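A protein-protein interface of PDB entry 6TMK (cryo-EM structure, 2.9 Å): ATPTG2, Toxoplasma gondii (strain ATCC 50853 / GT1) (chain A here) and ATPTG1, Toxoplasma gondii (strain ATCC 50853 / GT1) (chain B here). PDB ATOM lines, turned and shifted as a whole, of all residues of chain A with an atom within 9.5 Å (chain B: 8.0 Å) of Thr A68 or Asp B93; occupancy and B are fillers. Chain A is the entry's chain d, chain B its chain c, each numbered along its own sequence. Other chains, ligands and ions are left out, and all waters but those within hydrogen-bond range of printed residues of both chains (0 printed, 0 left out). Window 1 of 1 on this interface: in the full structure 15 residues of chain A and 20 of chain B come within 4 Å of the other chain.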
ATOM      1  N   GLY A  64     -38.966  -4.883  -9.887  1.00  0.00           N
ATOM      2  CA  GLY A  64     -37.623  -4.667  -9.406  1.00  0.00           C
ATOM      3  C   GLY A  64     -36.923  -5.966  -9.069  1.00  0.00           C
ATOM      4  O   GLY A  64     -37.542  -6.963  -8.699  1.00  0.00           O
ATOM      5  N   GLU A  65     -35.602  -5.946  -9.197  1.00  0.00           N
ATOM      6  CA  GLU A  65     -34.816  -7.137  -8.952  1.00  0.00           C
ATOM      7  C   GLU A  65     -34.868  -7.528  -7.479  1.00  0.00           C
ATOM      8  O   GLU A  65     -35.437  -6.834  -6.633  1.00  0.00           O
ATOM      9  CB  GLU A  65     -33.372  -6.936  -9.407  1.00  0.00           C
ATOM     10  CG  GLU A  65     -32.591  -5.852  -8.687  1.00  0.00           C
ATOM     11  CD  GLU A  65     -32.749  -4.495  -9.339  1.00  0.00           C
ATOM     12  OE1 GLU A  65     -33.723  -4.302 -10.095  1.00  0.00           O
ATOM     13  OE2 GLU A  65     -31.888  -3.623  -9.110  1.00  0.00           O
ATOM     14  N   HIS A  66     -34.261  -8.672  -7.188  1.00  0.00           N
ATOM     15  CA  HIS A  66     -34.089  -9.119  -5.817  1.00  0.00           C
ATOM     16  C   HIS A  66     -33.408  -8.055  -4.971  1.00  0.00           C
ATOM     17  O   HIS A  66     -32.511  -7.348  -5.433  1.00  0.00           O
ATOM     18  CB  HIS A  66     -33.251 -10.392  -5.811  1.00  0.00           C
ATOM     19  CG  HIS A  66     -33.600 -11.352  -4.722  1.00  0.00           C
ATOM     20  ND1 HIS A  66     -33.069 -11.262  -3.455  1.00  0.00           N
ATOM     21  CD2 HIS A  66     -34.404 -12.438  -4.717  1.00  0.00           C
ATOM     22  CE1 HIS A  66     -33.542 -12.244  -2.714  1.00  0.00           C
ATOM     23  NE2 HIS A  66     -34.356 -12.971  -3.455  1.00  0.00           N
ATOM     24  N   ALA A  67     -33.837  -7.956  -3.715  1.00  0.00           N
ATOM     25  CA  ALA A  67     -33.328  -6.908  -2.846  1.00  0.00           C
ATOM     26  C   ALA A  67     -31.921  -7.221  -2.358  1.00  0.00           C
ATOM     27  O   ALA A  67     -31.094  -6.314  -2.218  1.00  0.00           O
ATOM     28  CB  ALA A  67     -34.269  -6.716  -1.662  1.00  0.00           C
ATOM     29  N   THR A  68     -31.630  -8.493  -2.095  1.00  0.00           N
ATOM     30  CA  THR A  68     -30.374  -8.886  -1.477  1.00  0.00           C
ATOM     31  C   THR A  68     -29.427  -9.613  -2.417  1.00  0.00           C
ATOM     32  O   THR A  68     -28.215  -9.549  -2.213  1.00  0.00           O
ATOM     33  CB  THR A  68     -30.643  -9.764  -0.249  1.00  0.00           C
ATOM     34  OG1 THR A  68     -29.411 -10.261   0.280  1.00  0.00           O
ATOM     35  CG2 THR A  68     -31.529 -10.904  -0.591  1.00  0.00           C
ATOM     36  N   TYR A  69     -29.941 -10.304  -3.429  1.00  0.00           N
ATOM     37  CA  TYR A  69     -29.117 -10.941  -4.452  1.00  0.00           C
ATOM     38  C   TYR A  69     -29.420 -10.241  -5.769  1.00  0.00           C
ATOM     39  O   TYR A  69     -30.187 -10.730  -6.595  1.00  0.00           O
ATOM     40  CB  TYR A  69     -29.380 -12.428  -4.544  1.00  0.00           C
ATOM     41  CG  TYR A  69     -29.182 -13.161  -3.251  1.00  0.00           C
ATOM     42  CD1 TYR A  69     -27.973 -13.117  -2.589  1.00  0.00           C
ATOM     43  CD2 TYR A  69     -30.204 -13.901  -2.692  1.00  0.00           C
ATOM     44  CE1 TYR A  69     -27.790 -13.778  -1.409  1.00  0.00           C
ATOM     45  CE2 TYR A  69     -30.028 -14.567  -1.513  1.00  0.00           C
ATOM     46  CZ  TYR A  69     -28.819 -14.502  -0.874  1.00  0.00           C
ATOM     47  OH  TYR A  69     -28.640 -15.169   0.311  1.00  0.00           O
ATOM     48  N   ASN A  70     -28.783  -9.102  -5.972  1.00  0.00           N
ATOM     49  CA  ASN A  70     -29.041  -8.272  -7.130  1.00  0.00           C
ATOM     50  C   ASN A  70     -27.859  -8.302  -8.092  1.00  0.00           C
ATOM     51  O   ASN A  70     -26.789  -8.865  -7.819  1.00  0.00           O
ATOM     52  CB  ASN A  70     -29.381  -6.845  -6.700  1.00  0.00           C
ATOM     53  CG  ASN A  70     -28.280  -6.191  -5.914  1.00  0.00           C
ATOM     54  OD1 ASN A  70     -27.195  -5.930  -6.428  1.00  0.00           O
ATOM     55  ND2 ASN A  70     -28.554  -5.910  -4.657  1.00  0.00           N
ATOM     56  N   TYR A  71     -28.071  -7.640  -9.227  1.00  0.00           N
ATOM     57  CA  TYR A  71     -27.150  -7.751 -10.346  1.00  0.00           C
ATOM     58  C   TYR A  71     -25.788  -7.192  -9.979  1.00  0.00           C
ATOM     59  O   TYR A  71     -24.755  -7.830 -10.210  1.00  0.00           O
ATOM     60  CB  TYR A  71     -27.721  -7.012 -11.553  1.00  0.00           C
ATOM     61  CG  TYR A  71     -29.169  -7.306 -11.845  1.00  0.00           C
ATOM     62  CD1 TYR A  71     -29.634  -8.603 -11.946  1.00  0.00           C
ATOM     63  CD2 TYR A  71     -30.074  -6.277 -12.015  1.00  0.00           C
ATOM     64  CE1 TYR A  71     -30.957  -8.860 -12.210  1.00  0.00           C
ATOM     65  CE2 TYR A  71     -31.392  -6.527 -12.279  1.00  0.00           C
ATOM     66  CZ  TYR A  71     -31.830  -7.816 -12.377  1.00  0.00           C
ATOM     67  OH  TYR A  71     -33.154  -8.049 -12.640  1.00  0.00           O
ATOM     68  N   PHE A  72     -25.768  -6.003  -9.382  1.00  0.00           N
ATOM     69  CA  PHE A  72     -24.499  -5.362  -9.089  1.00  0.00           C
ATOM     70  C   PHE A  72     -23.722  -6.121  -8.029  1.00  0.00           C
ATOM     71  O   PHE A  72     -22.497  -6.235  -8.117  1.00  0.00           O
ATOM     72  CB  PHE A  72     -24.700  -3.929  -8.630  1.00  0.00           C
ATOM     73  CG  PHE A  72     -23.432  -3.281  -8.205  1.00  0.00           C
ATOM     74  CD1 PHE A  72     -22.533  -2.832  -9.143  1.00  0.00           C
ATOM     75  CD2 PHE A  72     -23.110  -3.170  -6.871  1.00  0.00           C
ATOM     76  CE1 PHE A  72     -21.359  -2.262  -8.763  1.00  0.00           C
ATOM     77  CE2 PHE A  72     -21.937  -2.600  -6.488  1.00  0.00           C
ATOM     78  CZ  PHE A  72     -21.056  -2.145  -7.437  1.00  0.00           C
ATOM     79  N   VAL A  73     -24.401  -6.603  -6.992  1.00  0.00           N
ATOM     80  CA  VAL A  73     -23.672  -7.243  -5.912  1.00  0.00           C
ATOM     81  C   VAL A  73     -23.110  -8.576  -6.383  1.00  0.00           C
ATOM     82  O   VAL A  73     -21.968  -8.927  -6.068  1.00  0.00           O
ATOM     83  CB  VAL A  73     -24.567  -7.392  -4.668  1.00  0.00           C
ATOM     84  CG1 VAL A  73     -25.544  -8.517  -4.825  1.00  0.00           C
ATOM     85  CG2 VAL A  73     -23.738  -7.556  -3.427  1.00  0.00           C
ATOM     86  N   LEU A  74     -23.870  -9.311  -7.202  1.00  0.00           N
ATOM     87  CA  LEU A  74     -23.313 -10.521  -7.796  1.00  0.00           C
ATOM     88  C   LEU A  74     -22.135 -10.200  -8.712  1.00  0.00           C
ATOM     89  O   LEU A  74     -21.111 -10.895  -8.694  1.00  0.00           O
ATOM     90  CB  LEU A  74     -24.401 -11.269  -8.558  1.00  0.00           C
ATOM     91  CG  LEU A  74     -25.567 -11.803  -7.730  1.00  0.00           C
ATOM     92  CD1 LEU A  74     -26.631 -12.380  -8.613  1.00  0.00           C
ATOM     93  CD2 LEU A  74     -25.118 -12.833  -6.736  1.00  0.00           C
ATOM     94  N   PHE A  75     -22.249  -9.131  -9.497  1.00  0.00           N
ATOM     95  CA  PHE A  75     -21.179  -8.739 -10.404  1.00  0.00           C
ATOM     96  C   PHE A  75     -19.900  -8.404  -9.645  1.00  0.00           C
ATOM     97  O   PHE A  75     -18.813  -8.891  -9.983  1.00  0.00           O
ATOM     98  CB  PHE A  75     -21.646  -7.557 -11.253  1.00  0.00           C
ATOM     99  CG  PHE A  75     -20.599  -7.012 -12.164  1.00  0.00           C
ATOM    100  CD1 PHE A  75     -20.207  -7.710 -13.283  1.00  0.00           C
ATOM    101  CD2 PHE A  75     -20.015  -5.792 -11.908  1.00  0.00           C
ATOM    102  CE1 PHE A  75     -19.248  -7.211 -14.118  1.00  0.00           C
ATOM    103  CE2 PHE A  75     -19.055  -5.290 -12.741  1.00  0.00           C
ATOM    104  CZ  PHE A  75     -18.671  -5.999 -13.849  1.00  0.00           C
ATOM    105  N   ARG A  77     -19.083  -9.187  -6.603  1.00  0.00           N
ATOM    106  CA  ARG A  77     -18.563 -10.381  -5.957  1.00  0.00           C
ATOM    107  C   ARG A  77     -17.810 -11.263  -6.939  1.00  0.00           C
ATOM    108  O   ARG A  77     -16.860 -11.951  -6.551  1.00  0.00           O
ATOM    109  CB  ARG A  77     -19.696 -11.144  -5.289  1.00  0.00           C
ATOM    110  CG  ARG A  77     -20.177 -10.471  -4.038  1.00  0.00           C
ATOM    111  CD  ARG A  77     -21.373 -11.129  -3.433  1.00  0.00           C
ATOM    112  NE  ARG A  77     -21.963 -10.291  -2.404  1.00  0.00           N
ATOM    113  CZ  ARG A  77     -23.039 -10.610  -1.700  1.00  0.00           C
ATOM    114  NH1 ARG A  77     -23.646 -11.759  -1.896  1.00  0.00           N
ATOM    115  NH2 ARG A  77     -23.496  -9.781  -0.783  1.00  0.00           N
ATOM    116  N   LEU B  88     -37.546 -19.066  -3.778  1.00  0.00           N
ATOM    117  CA  LEU B  88     -37.019 -17.799  -3.304  1.00  0.00           C
ATOM    118  C   LEU B  88     -36.284 -17.960  -1.981  1.00  0.00           C
ATOM    119  O   LEU B  88     -36.738 -18.659  -1.071  1.00  0.00           O
ATOM    120  CB  LEU B  88     -38.155 -16.798  -3.159  1.00  0.00           C
ATOM    121  CG  LEU B  88     -37.801 -15.358  -2.832  1.00  0.00           C
ATOM    122  CD1 LEU B  88     -37.295 -14.659  -4.060  1.00  0.00           C
ATOM    123  CD2 LEU B  88     -39.019 -14.672  -2.320  1.00  0.00           C
ATOM    124  N   VAL B  89     -35.135 -17.298  -1.885  1.00  0.00           N
ATOM    125  CA  VAL B  89     -34.392 -17.130  -0.646  1.00  0.00           C
ATOM    126  C   VAL B  89     -34.242 -15.640  -0.389  1.00  0.00           C
ATOM    127  O   VAL B  89     -33.991 -14.861  -1.313  1.00  0.00           O
ATOM    128  CB  VAL B  89     -33.014 -17.820  -0.708  1.00  0.00           C
ATOM    129  CG1 VAL B  89     -32.267 -17.632   0.584  1.00  0.00           C
ATOM    130  CG2 VAL B  89     -33.177 -19.280  -0.988  1.00  0.00           C
ATOM    131  N   GLU B  90     -34.407 -15.249   0.872  1.00  0.00           N
ATOM    132  CA  GLU B  90     -34.468 -13.849   1.261  1.00  0.00           C
ATOM    133  C   GLU B  90     -33.206 -13.328   1.932  1.00  0.00           C
ATOM    134  O   GLU B  90     -33.009 -12.110   1.964  1.00  0.00           O
ATOM    135  CB  GLU B  90     -35.641 -13.628   2.221  1.00  0.00           C
ATOM    136  CG  GLU B  90     -37.005 -13.844   1.613  1.00  0.00           C
ATOM    137  CD  GLU B  90     -37.669 -15.114   2.095  1.00  0.00           C
ATOM    138  OE1 GLU B  90     -36.963 -16.127   2.274  1.00  0.00           O
ATOM    139  OE2 GLU B  90     -38.901 -15.101   2.291  1.00  0.00           O
ATOM    140  N   GLY B  91     -32.344 -14.200   2.454  1.00  0.00           N
ATOM    141  CA  GLY B  91     -31.422 -13.838   3.506  1.00  0.00           C
ATOM    142  C   GLY B  91     -30.031 -13.458   3.024  1.00  0.00           C
ATOM    143  O   GLY B  91     -29.726 -13.419   1.836  1.00  0.00           O
ATOM    144  N   ALA B  92     -29.173 -13.188   4.008  1.00  0.00           N
ATOM    145  CA  ALA B  92     -27.744 -12.965   3.806  1.00  0.00           C
ATOM    146  C   ALA B  92     -27.489 -11.748   2.911  1.00  0.00           C
ATOM    147  O   ALA B  92     -27.060 -11.846   1.761  1.00  0.00           O
ATOM    148  CB  ALA B  92     -27.081 -14.220   3.227  1.00  0.00           C
ATOM    149  N   ASP B  93     -27.785 -10.580   3.488  1.00  0.00           N
ATOM    150  CA  ASP B  93     -27.291  -9.328   2.925  1.00  0.00           C
ATOM    151  C   ASP B  93     -25.781  -9.355   2.733  1.00  0.00           C
ATOM    152  O   ASP B  93     -25.247  -8.628   1.889  1.00  0.00           O
ATOM    153  CB  ASP B  93     -27.679  -8.160   3.829  1.00  0.00           C
ATOM    154  CG  ASP B  93     -28.942  -7.455   3.374  1.00  0.00           C
ATOM    155  OD1 ASP B  93     -29.661  -7.995   2.507  1.00  0.00           O
ATOM    156  OD2 ASP B  93     -29.217  -6.352   3.893  1.00  0.00           O
ATOM    157  N   PHE B  94     -25.079 -10.163   3.517  1.00  0.00           N
ATOM    158  CA  PHE B  94     -23.643 -10.363   3.420  1.00  0.00           C
ATOM    159  C   PHE B  94     -23.369 -11.764   2.887  1.00  0.00           C
ATOM    160  O   PHE B  94     -24.288 -12.546   2.640  1.00  0.00           O
ATOM    161  CB  PHE B  94     -22.991 -10.137   4.782  1.00  0.00           C
ATOM    162  CG  PHE B  94     -23.393 -11.137   5.813  1.00  0.00           C
ATOM    163  CD1 PHE B  94     -24.566 -10.986   6.519  1.00  0.00           C
ATOM    164  CD2 PHE B  94     -22.596 -12.225   6.084  1.00  0.00           C
ATOM    165  CE1 PHE B  94     -24.938 -11.903   7.460  1.00  0.00           C
ATOM    166  CE2 PHE B  94     -22.965 -13.143   7.024  1.00  0.00           C
ATOM    167  CZ  PHE B  94     -24.137 -12.979   7.717  1.00  0.00           C
ATOM    168  N   TYR B  95     -22.090 -12.089   2.707  1.00  0.00           N
ATOM    169  CA  TYR B  95     -21.734 -13.421   2.248  1.00  0.00           C
ATOM    170  C   TYR B  95     -20.378 -13.771   2.838  1.00  0.00           C
ATOM    171  O   TYR B  95     -19.716 -12.940   3.462  1.00  0.00           O
ATOM    172  CB  TYR B  95     -21.698 -13.482   0.723  1.00  0.00           C
ATOM    173  CG  TYR B  95     -20.515 -12.807   0.084  1.00  0.00           C
ATOM    174  CD1 TYR B  95     -20.399 -11.434   0.027  1.00  0.00           C
ATOM    175  CD2 TYR B  95     -19.567 -13.564  -0.574  1.00  0.00           C
ATOM    176  CE1 TYR B  95     -19.316 -10.845  -0.580  1.00  0.00           C
ATOM    177  CE2 TYR B  95     -18.496 -12.989  -1.184  1.00  0.00           C
ATOM    178  CZ  TYR B  95     -18.380 -11.633  -1.206  1.00  0.00           C
ATOM    179  OH  TYR B  95     -17.290 -11.085  -1.831  1.00  0.00           O
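Of the 8 printed residues of chain B, 7 touch a printed residue of chain A.
Of the 13 printed residues of chain A, 4 touch a printed residue of chain B.
Hydrophobic or aromatic side chains of chain A that line the printed part of chain B: His A66 and Tyr A69.
Among the printed residues, 11 pairs touch across the chains.
Among the printed residues, no Asp or Glu carboxylate lies within 4 Å of a Lys or Arg side-chain nitrogen of the other chain.
N of Thr A68 sits close to ND1 of His A66, at 3.4 Å.
The backbone NH (N) of Tyr A69 is in hydrogen-bond range of a ring nitrogen (ND1) of His A66 (3.3 Å).
Among the printed residues, pairs that only touch across the chains: His A66 with Leu B88 (3.4 Å), Thr A68 with Glu B90 (3.2 Å), Thr A68 with Gly B91 (3.5 Å), Tyr A69 with Val B89 (3.98 Å), Tyr A69 with Ala B92 (3.4 Å) and Arg A77 with Tyr B95 (3.1 Å).
OD1 of Asp B93 sits at hydrogen-bond distance from OG1 of Thr A68 (3.2 Å).
O of Ala B92 sits at hydrogen-bond distance from OG1 of Thr A68.
The backbone carbonyl oxygen (O) of Val B89 lies within hydrogen-bond range of a ring nitrogen (NE2) of His A66.
The backbone carbonyl oxygen of Gly B91 sits at hydrogen-bond distance from the side-chain hydroxyl of Tyr A69, 2.6 Å away.
The guanidinium group of Arg A77 lies within hydrogen-bond range of the backbone carbonyl oxygen of Asp B93.
Of chain B, only Glu B90, Gly B91, Ala B92 and Asp B93 come within 4 Å of Thr A68.
Gly B91 touches two residues of chain A.
Of chain A, only Thr A68 (3.2 Å) and Tyr A69 (3.4 Å) come within 4 Å of Ala B92.
Printed residues of chain A within 4 Å of Leu B88: His A66.
Of the printed residues of chain B, Tyr A69 touches Val B89 (3.98 Å), Gly B91 (2.6 Å) and Ala B92 (3.4 Å).
Printed residues of chain B within 4 Å of His A66: Leu B88 and Val B89.
The nearest printed residue of chain A that does not touch Glu B90 is His A66 (4.4 Å).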
